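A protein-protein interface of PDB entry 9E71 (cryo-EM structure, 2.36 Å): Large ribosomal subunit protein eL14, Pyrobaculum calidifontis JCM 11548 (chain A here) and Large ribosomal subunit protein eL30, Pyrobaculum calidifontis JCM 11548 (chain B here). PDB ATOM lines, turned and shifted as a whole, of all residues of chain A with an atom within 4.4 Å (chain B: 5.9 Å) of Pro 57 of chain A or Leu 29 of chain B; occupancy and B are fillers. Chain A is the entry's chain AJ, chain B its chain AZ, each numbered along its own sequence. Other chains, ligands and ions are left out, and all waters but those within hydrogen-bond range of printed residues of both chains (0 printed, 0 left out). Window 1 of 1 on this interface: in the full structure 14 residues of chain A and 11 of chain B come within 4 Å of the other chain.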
ATOM      1  N   LYS A   3      25.533  10.542 -31.582  1.00  0.00           N
ATOM      2  CA  LYS A   3      25.454   9.874 -30.290  1.00  0.00           C
ATOM      3  C   LYS A   3      26.369   8.653 -30.263  1.00  0.00           C
ATOM      4  O   LYS A   3      26.566   7.994 -31.281  1.00  0.00           O
ATOM      5  CB  LYS A   3      24.013   9.465 -29.984  1.00  0.00           C
ATOM      6  CG  LYS A   3      23.716   8.002 -30.264  1.00  0.00           C
ATOM      7  CD  LYS A   3      22.431   7.560 -29.593  1.00  0.00           C
ATOM      8  CE  LYS A   3      21.247   8.345 -30.121  1.00  0.00           C
ATOM      9  NZ  LYS A   3      21.188   8.301 -31.606  1.00  0.00           N
ATOM     10  N   VAL A   4      26.929   8.355 -29.096  1.00  0.00           N
ATOM     11  CA  VAL A   4      27.854   7.234 -28.969  1.00  0.00           C
ATOM     12  C   VAL A   4      27.133   5.959 -28.556  1.00  0.00           C
ATOM     13  O   VAL A   4      27.346   4.900 -29.150  1.00  0.00           O
ATOM     14  CB  VAL A   4      28.976   7.585 -27.974  1.00  0.00           C
ATOM     15  CG1 VAL A   4      29.843   6.373 -27.716  1.00  0.00           C
ATOM     16  CG2 VAL A   4      29.812   8.725 -28.509  1.00  0.00           C
ATOM     17  N   ILE A   5      26.282   6.036 -27.536  1.00  0.00           N
ATOM     18  CA  ILE A   5      25.592   4.858 -27.014  1.00  0.00           C
ATOM     19  C   ILE A   5      24.367   4.662 -27.900  1.00  0.00           C
ATOM     20  O   ILE A   5      23.334   5.306 -27.731  1.00  0.00           O
ATOM     21  CB  ILE A   5      25.240   5.007 -25.540  1.00  0.00           C
ATOM     22  CG1 ILE A   5      26.496   4.818 -24.691  1.00  0.00           C
ATOM     23  CG2 ILE A   5      24.190   4.000 -25.137  1.00  0.00           C
ATOM     24  CD1 ILE A   5      26.951   3.385 -24.597  1.00  0.00           C
ATOM     25  N   ARG A   9      26.307  -0.810 -30.949  1.00  0.00           N
ATOM     26  CA  ARG A   9      27.554  -0.404 -30.319  1.00  0.00           C
ATOM     27  C   ARG A   9      28.042  -1.479 -29.358  1.00  0.00           C
ATOM     28  O   ARG A   9      27.258  -2.075 -28.614  1.00  0.00           O
ATOM     29  CB  ARG A   9      27.373   0.918 -29.578  1.00  0.00           C
ATOM     30  CG  ARG A   9      28.450   1.199 -28.549  1.00  0.00           C
ATOM     31  CD  ARG A   9      29.715   1.732 -29.194  1.00  0.00           C
ATOM     32  NE  ARG A   9      29.456   2.945 -29.956  1.00  0.00           N
ATOM     33  CZ  ARG A   9      30.319   3.505 -30.791  1.00  0.00           C
ATOM     34  NH1 ARG A   9      31.531   3.009 -30.968  1.00  0.00           N
ATOM     35  NH2 ARG A   9      29.957   4.594 -31.462  1.00  0.00           N
ATOM     36  N   VAL A  10      29.342  -1.729 -29.386  1.00  0.00           N
ATOM     37  CA  VAL A  10      29.976  -2.664 -28.470  1.00  0.00           C
ATOM     38  C   VAL A  10      30.393  -1.904 -27.217  1.00  0.00           C
ATOM     39  O   VAL A  10      31.139  -0.921 -27.293  1.00  0.00           O
ATOM     40  CB  VAL A  10      31.181  -3.348 -29.130  1.00  0.00           C
ATOM     41  CG1 VAL A  10      31.838  -4.306 -28.163  1.00  0.00           C
ATOM     42  CG2 VAL A  10      30.749  -4.065 -30.382  1.00  0.00           C
ATOM     43  N   VAL A  11      29.910  -2.360 -26.063  1.00  0.00           N
ATOM     44  CA  VAL A  11      30.178  -1.707 -24.790  1.00  0.00           C
ATOM     45  C   VAL A  11      30.728  -2.742 -23.822  1.00  0.00           C
ATOM     46  O   VAL A  11      30.643  -3.948 -24.051  1.00  0.00           O
ATOM     47  CB  VAL A  11      28.918  -1.036 -24.206  1.00  0.00           C
ATOM     48  CG1 VAL A  11      28.281  -0.127 -25.236  1.00  0.00           C
ATOM     49  CG2 VAL A  11      27.930  -2.086 -23.746  1.00  0.00           C
ATOM     50  N   ILE A  52      23.253   3.739 -18.544  1.00  0.00           N
ATOM     51  CA  ILE A  52      24.342   4.094 -19.447  1.00  0.00           C
ATOM     52  C   ILE A  52      25.589   4.517 -18.688  1.00  0.00           C
ATOM     53  O   ILE A  52      26.695   4.452 -19.233  1.00  0.00           O
ATOM     54  CB  ILE A  52      23.908   5.193 -20.435  1.00  0.00           C
ATOM     55  CG1 ILE A  52      23.922   6.562 -19.757  1.00  0.00           C
ATOM     56  CG2 ILE A  52      22.545   4.885 -21.012  1.00  0.00           C
ATOM     57  CD1 ILE A  52      24.292   7.686 -20.695  1.00  0.00           C
ATOM     58  N   ILE A  55      28.099   1.436 -18.262  1.00  0.00           N
ATOM     59  CA  ILE A  55      28.700   0.825 -19.440  1.00  0.00           C
ATOM     60  C   ILE A  55      29.694   1.805 -20.035  1.00  0.00           C
ATOM     61  O   ILE A  55      29.458   3.018 -20.038  1.00  0.00           O
ATOM     62  CB  ILE A  55      27.648   0.437 -20.497  1.00  0.00           C
ATOM     63  CG1 ILE A  55      26.748   1.632 -20.804  1.00  0.00           C
ATOM     64  CG2 ILE A  55      26.842  -0.765 -20.036  1.00  0.00           C
ATOM     65  CD1 ILE A  55      25.950   1.477 -22.061  1.00  0.00           C
ATOM     66  N   GLU A  56      30.807   1.282 -20.533  1.00  0.00           N
ATOM     67  CA  GLU A  56      31.805   2.103 -21.196  1.00  0.00           C
ATOM     68  C   GLU A  56      31.832   1.757 -22.674  1.00  0.00           C
ATOM     69  O   GLU A  56      32.175   0.620 -23.027  1.00  0.00           O
ATOM     70  CB  GLU A  56      33.180   1.892 -20.571  1.00  0.00           C
ATOM     71  CG  GLU A  56      34.293   2.654 -21.264  1.00  0.00           C
ATOM     72  CD  GLU A  56      34.405   4.083 -20.784  1.00  0.00           C
ATOM     73  OE1 GLU A  56      33.467   4.565 -20.118  1.00  0.00           O
ATOM     74  OE2 GLU A  56      35.437   4.723 -21.069  1.00  0.00           O
ATOM     75  N   PRO A  57      31.477   2.679 -23.563  1.00  0.00           N
ATOM     76  CA  PRO A  57      31.482   2.358 -24.991  1.00  0.00           C
ATOM     77  C   PRO A  57      32.891   2.200 -25.527  1.00  0.00           C
ATOM     78  O   PRO A  57      33.822   2.896 -25.118  1.00  0.00           O
ATOM     79  CB  PRO A  57      30.783   3.564 -25.621  1.00  0.00           C
ATOM     80  CG  PRO A  57      31.138   4.680 -24.719  1.00  0.00           C
ATOM     81  CD  PRO A  57      31.165   4.097 -23.326  1.00  0.00           C
ATOM     82  N   THR A  58      33.037   1.270 -26.457  1.00  0.00           N
ATOM     83  CA  THR A  58      34.284   1.057 -27.170  1.00  0.00           C
ATOM     84  C   THR A  58      34.245   1.783 -28.510  1.00  0.00           C
ATOM     85  O   THR A  58      33.239   2.377 -28.897  1.00  0.00           O
ATOM     86  CB  THR A  58      34.529  -0.435 -27.387  1.00  0.00           C
ATOM     87  OG1 THR A  58      33.507  -0.957 -28.241  1.00  0.00           O
ATOM     88  CG2 THR A  58      34.489  -1.173 -26.069  1.00  0.00           C
ATOM     89  N   THR B  24      27.108  16.943 -19.109  1.00  0.00           N
ATOM     90  CA  THR B  24      27.896  17.013 -20.335  1.00  0.00           C
ATOM     91  C   THR B  24      28.248  15.623 -20.845  1.00  0.00           C
ATOM     92  O   THR B  24      28.178  15.361 -22.051  1.00  0.00           O
ATOM     93  CB  THR B  24      29.165  17.829 -20.095  1.00  0.00           C
ATOM     94  OG1 THR B  24      28.814  19.167 -19.723  1.00  0.00           O
ATOM     95  CG2 THR B  24      30.018  17.862 -21.345  1.00  0.00           C
ATOM     96  N   LYS B  25      28.617  14.716 -19.937  1.00  0.00           N
ATOM     97  CA  LYS B  25      28.932  13.348 -20.330  1.00  0.00           C
ATOM     98  C   LYS B  25      27.710  12.639 -20.897  1.00  0.00           C
ATOM     99  O   LYS B  25      27.804  11.934 -21.907  1.00  0.00           O
ATOM    100  CB  LYS B  25      29.517  12.594 -19.130  1.00  0.00           C
ATOM    101  CG  LYS B  25      29.238  11.091 -19.036  1.00  0.00           C
ATOM    102  CD  LYS B  25      27.957  10.753 -18.264  1.00  0.00           C
ATOM    103  CE  LYS B  25      28.021  11.217 -16.825  1.00  0.00           C
ATOM    104  NZ  LYS B  25      26.660  11.256 -16.231  1.00  0.00           N
ATOM    105  N   LYS B  26      26.552  12.811 -20.258  1.00  0.00           N
ATOM    106  CA  LYS B  26      25.347  12.160 -20.763  1.00  0.00           C
ATOM    107  C   LYS B  26      24.909  12.746 -22.098  1.00  0.00           C
ATOM    108  O   LYS B  26      24.440  12.008 -22.969  1.00  0.00           O
ATOM    109  CB  LYS B  26      24.219  12.264 -19.741  1.00  0.00           C
ATOM    110  CG  LYS B  26      23.368  11.017 -19.649  1.00  0.00           C
ATOM    111  CD  LYS B  26      23.824  10.128 -18.507  1.00  0.00           C
ATOM    112  CE  LYS B  26      22.692   9.242 -18.011  1.00  0.00           C
ATOM    113  NZ  LYS B  26      23.012   8.600 -16.707  1.00  0.00           N
ATOM    114  N   SER B  27      25.050  14.062 -22.280  1.00  0.00           N
ATOM    115  CA  SER B  27      24.707  14.676 -23.558  1.00  0.00           C
ATOM    116  C   SER B  27      25.655  14.222 -24.654  1.00  0.00           C
ATOM    117  O   SER B  27      25.254  14.080 -25.812  1.00  0.00           O
ATOM    118  CB  SER B  27      24.730  16.195 -23.438  1.00  0.00           C
ATOM    119  OG  SER B  27      23.810  16.775 -24.341  1.00  0.00           O
ATOM    120  N   LEU B  28      26.921  14.013 -24.311  1.00  0.00           N
ATOM    121  CA  LEU B  28      27.869  13.504 -25.287  1.00  0.00           C
ATOM    122  C   LEU B  28      27.561  12.055 -25.647  1.00  0.00           C
ATOM    123  O   LEU B  28      27.703  11.650 -26.805  1.00  0.00           O
ATOM    124  CB  LEU B  28      29.281  13.630 -24.732  1.00  0.00           C
ATOM    125  CG  LEU B  28      30.355  13.999 -25.744  1.00  0.00           C
ATOM    126  CD1 LEU B  28      31.636  14.411 -25.028  1.00  0.00           C
ATOM    127  CD2 LEU B  28      30.591  12.897 -26.739  1.00  0.00           C
ATOM    128  N   LEU B  29      27.157  11.253 -24.660  1.00  0.00           N
ATOM    129  CA  LEU B  29      26.905   9.840 -24.910  1.00  0.00           C
ATOM    130  C   LEU B  29      25.606   9.609 -25.670  1.00  0.00           C
ATOM    131  O   LEU B  29      25.554   8.752 -26.559  1.00  0.00           O
ATOM    132  CB  LEU B  29      26.876   9.063 -23.593  1.00  0.00           C
ATOM    133  CG  LEU B  29      28.205   8.586 -23.010  1.00  0.00           C
ATOM    134  CD1 LEU B  29      28.050   8.296 -21.526  1.00  0.00           C
ATOM    135  CD2 LEU B  29      28.706   7.357 -23.749  1.00  0.00           C
ATOM    136  N   THR B  30      24.548  10.336 -25.334  1.00  0.00           N
ATOM    137  CA  THR B  30      23.233  10.058 -25.900  1.00  0.00           C
ATOM    138  C   THR B  30      22.734  11.135 -26.844  1.00  0.00           C
ATOM    139  O   THR B  30      22.120  10.819 -27.865  1.00  0.00           O
ATOM    140  CB  THR B  30      22.203   9.860 -24.780  1.00  0.00           C
ATOM    141  OG1 THR B  30      22.440  10.810 -23.734  1.00  0.00           O
ATOM    142  CG2 THR B  30      22.297   8.451 -24.218  1.00  0.00           C
ATOM    143  N   GLY B  31      22.971  12.398 -26.533  1.00  0.00           N
ATOM    144  CA  GLY B  31      22.562  13.490 -27.384  1.00  0.00           C
ATOM    145  C   GLY B  31      23.588  13.773 -28.454  1.00  0.00           C
ATOM    146  O   GLY B  31      24.469  12.960 -28.744  1.00  0.00           O
ATOM    147  N   TYR B  52      37.771  11.184 -24.656  1.00  0.00           N
ATOM    148  CA  TYR B  52      37.431   9.903 -25.269  1.00  0.00           C
ATOM    149  C   TYR B  52      36.007   9.904 -25.808  1.00  0.00           C
ATOM    150  O   TYR B  52      35.758   9.475 -26.945  1.00  0.00           O
ATOM    151  CB  TYR B  52      37.615   8.781 -24.251  1.00  0.00           C
ATOM    152  CG  TYR B  52      37.286   7.409 -24.785  1.00  0.00           C
ATOM    153  CD1 TYR B  52      38.072   6.814 -25.760  1.00  0.00           C
ATOM    154  CD2 TYR B  52      36.181   6.713 -24.321  1.00  0.00           C
ATOM    155  CE1 TYR B  52      37.768   5.562 -26.250  1.00  0.00           C
ATOM    156  CE2 TYR B  52      35.871   5.469 -24.804  1.00  0.00           C
ATOM    157  CZ  TYR B  52      36.667   4.895 -25.767  1.00  0.00           C
ATOM    158  OH  TYR B  52      36.358   3.648 -26.247  1.00  0.00           O
ATOM    159  N   TYR B  53      35.056  10.403 -25.012  1.00  0.00           N
ATOM    160  CA  TYR B  53      33.670  10.412 -25.465  1.00  0.00           C
ATOM    161  C   TYR B  53      33.479  11.356 -26.644  1.00  0.00           C
ATOM    162  O   TYR B  53      32.776  11.018 -27.603  1.00  0.00           O
ATOM    163  CB  TYR B  53      32.744  10.795 -24.314  1.00  0.00           C
ATOM    164  CG  TYR B  53      32.665   9.736 -23.247  1.00  0.00           C
ATOM    165  CD1 TYR B  53      32.903   8.407 -23.552  1.00  0.00           C
ATOM    166  CD2 TYR B  53      32.371  10.064 -21.931  1.00  0.00           C
ATOM    167  CE1 TYR B  53      32.844   7.433 -22.586  1.00  0.00           C
ATOM    168  CE2 TYR B  53      32.310   9.094 -20.955  1.00  0.00           C
ATOM    169  CZ  TYR B  53      32.547   7.777 -21.291  1.00  0.00           C
ATOM    170  OH  TYR B  53      32.487   6.798 -20.329  1.00  0.00           O
ATOM    171  N   LEU B  56      34.805   9.810 -29.762  1.00  0.00           N
ATOM    172  CA  LEU B  56      33.887   8.804 -30.289  1.00  0.00           C
ATOM    173  C   LEU B  56      32.696   9.447 -30.991  1.00  0.00           C
ATOM    174  O   LEU B  56      32.313   9.027 -32.086  1.00  0.00           O
ATOM    175  CB  LEU B  56      33.410   7.882 -29.170  1.00  0.00           C
ATOM    176  CG  LEU B  56      34.462   6.904 -28.661  1.00  0.00           C
ATOM    177  CD1 LEU B  56      33.807   5.737 -27.958  1.00  0.00           C
ATOM    178  CD2 LEU B  56      35.315   6.427 -29.810  1.00  0.00           C
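Printed residues of chain B within 4 Å of Pro 57 of chain A: Leu 29, Tyr 52 and Tyr 53. Of the printed residues of chain B, Lys 3 of chain A touches Leu 29 (3.8 Å), Thr 30 (3.1 Å) and Gly 31 (3.6 Å). Of the printed residues of chain A, Lys 26 of chain B touches Ile 52 (3.3 Å). Of the printed residues of chain B, Thr 58 of chain A touches Tyr 52 (3.4 Å) and Leu 56 (3.5 Å). Printed residues of chain B within 4 Å of Ile 5 of chain A: Leu 29 (3.0 Å). Of the printed residues of chain A, Tyr 52 of chain B touches Glu 56 (3.8 Å), Pro 57 (2.9 Å) and Thr 58 (3.4 Å). Lys 25 of chain B touches none of the printed residues of chain A. Arg 9 of chain A touches none of the printed residues of chain B. The nearest printed residue of chain B that does not touch Pro 57 of chain A is Leu 56 of chain B (4.02 Å). The nearest printed residue of chain A that does not touch Leu 29 of chain B is Ile 55 of chain A (5.7 Å).
N of Val 4 of chain A sits at hydrogen-bond distance from O of Leu 29 of chain B (2.9 Å). N of Ile 5 of chain A sits at hydrogen-bond distance from O of Leu 29 of chain B. The side-chain hydroxyl (OH) of Tyr 53 of chain B is in hydrogen-bond range of the side-chain carboxylate (OE1) of Glu 56 of chain A (2.4 Å). The side-chain hydroxyl of Tyr 52 of chain B is in hydrogen-bond range of the backbone carbonyl oxygen of Pro 57 of chain A (2.9 Å).
Of the 11 printed residues of chain B, 8 touch a printed residue of chain A. Along chain B the printed residues that touch a printed residue of chain A span positions 26 to 56. Among the printed residues, no Asp or Glu carboxylate lies within 4 Å of a Lys or Arg side-chain nitrogen of the other chain.
Among the printed residues, merely in contact across the chains: Lys 3 of chain A with Leu 29 of chain B (3.8 Å), Lys 3 of chain A with Thr 30 of chain B (3.1 Å), Lys 3 of chain A with Gly 31 of chain B (3.6 Å), Val 4 of chain A with Leu 28 of chain B (3.99 Å), Val 4 of chain A with Tyr 53 of chain B (3.9 Å), Val 4 of chain A with Leu 56 of chain B (3.8 Å), Ile 52 of chain A with Lys 26 of chain B (3.3 Å), Ile 52 of chain A with Leu 29 of chain B (3.9 Å), Glu 56 of chain A with Tyr 52 of chain B (3.8 Å), Pro 57 of chain A with Leu 29 of chain B (3.7 Å), Pro 57 of chain A with Tyr 53 of chain B (3.8 Å), Thr 58 of chain A with Tyr 52 of chain B (3.4 Å) and Thr 58 of chain A with Leu 56 of chain B (3.5 Å).
The backbone carbonyl oxygen (O) of Val 4 of chain A sits at hydrogen-bond distance from the guanidinium group (NE) of Arg 9 of chain A. NH1 of Arg 9 of chain A is in hydrogen-bond range of O of Thr 58 of chain A. OG1 of Thr 58 of chain A lies within hydrogen-bond range of O of Val 10 of chain A. O of Lys 26 of chain B is in hydrogen-bond range of OG1 of Thr 30 of chain B, 2.5 Å away.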
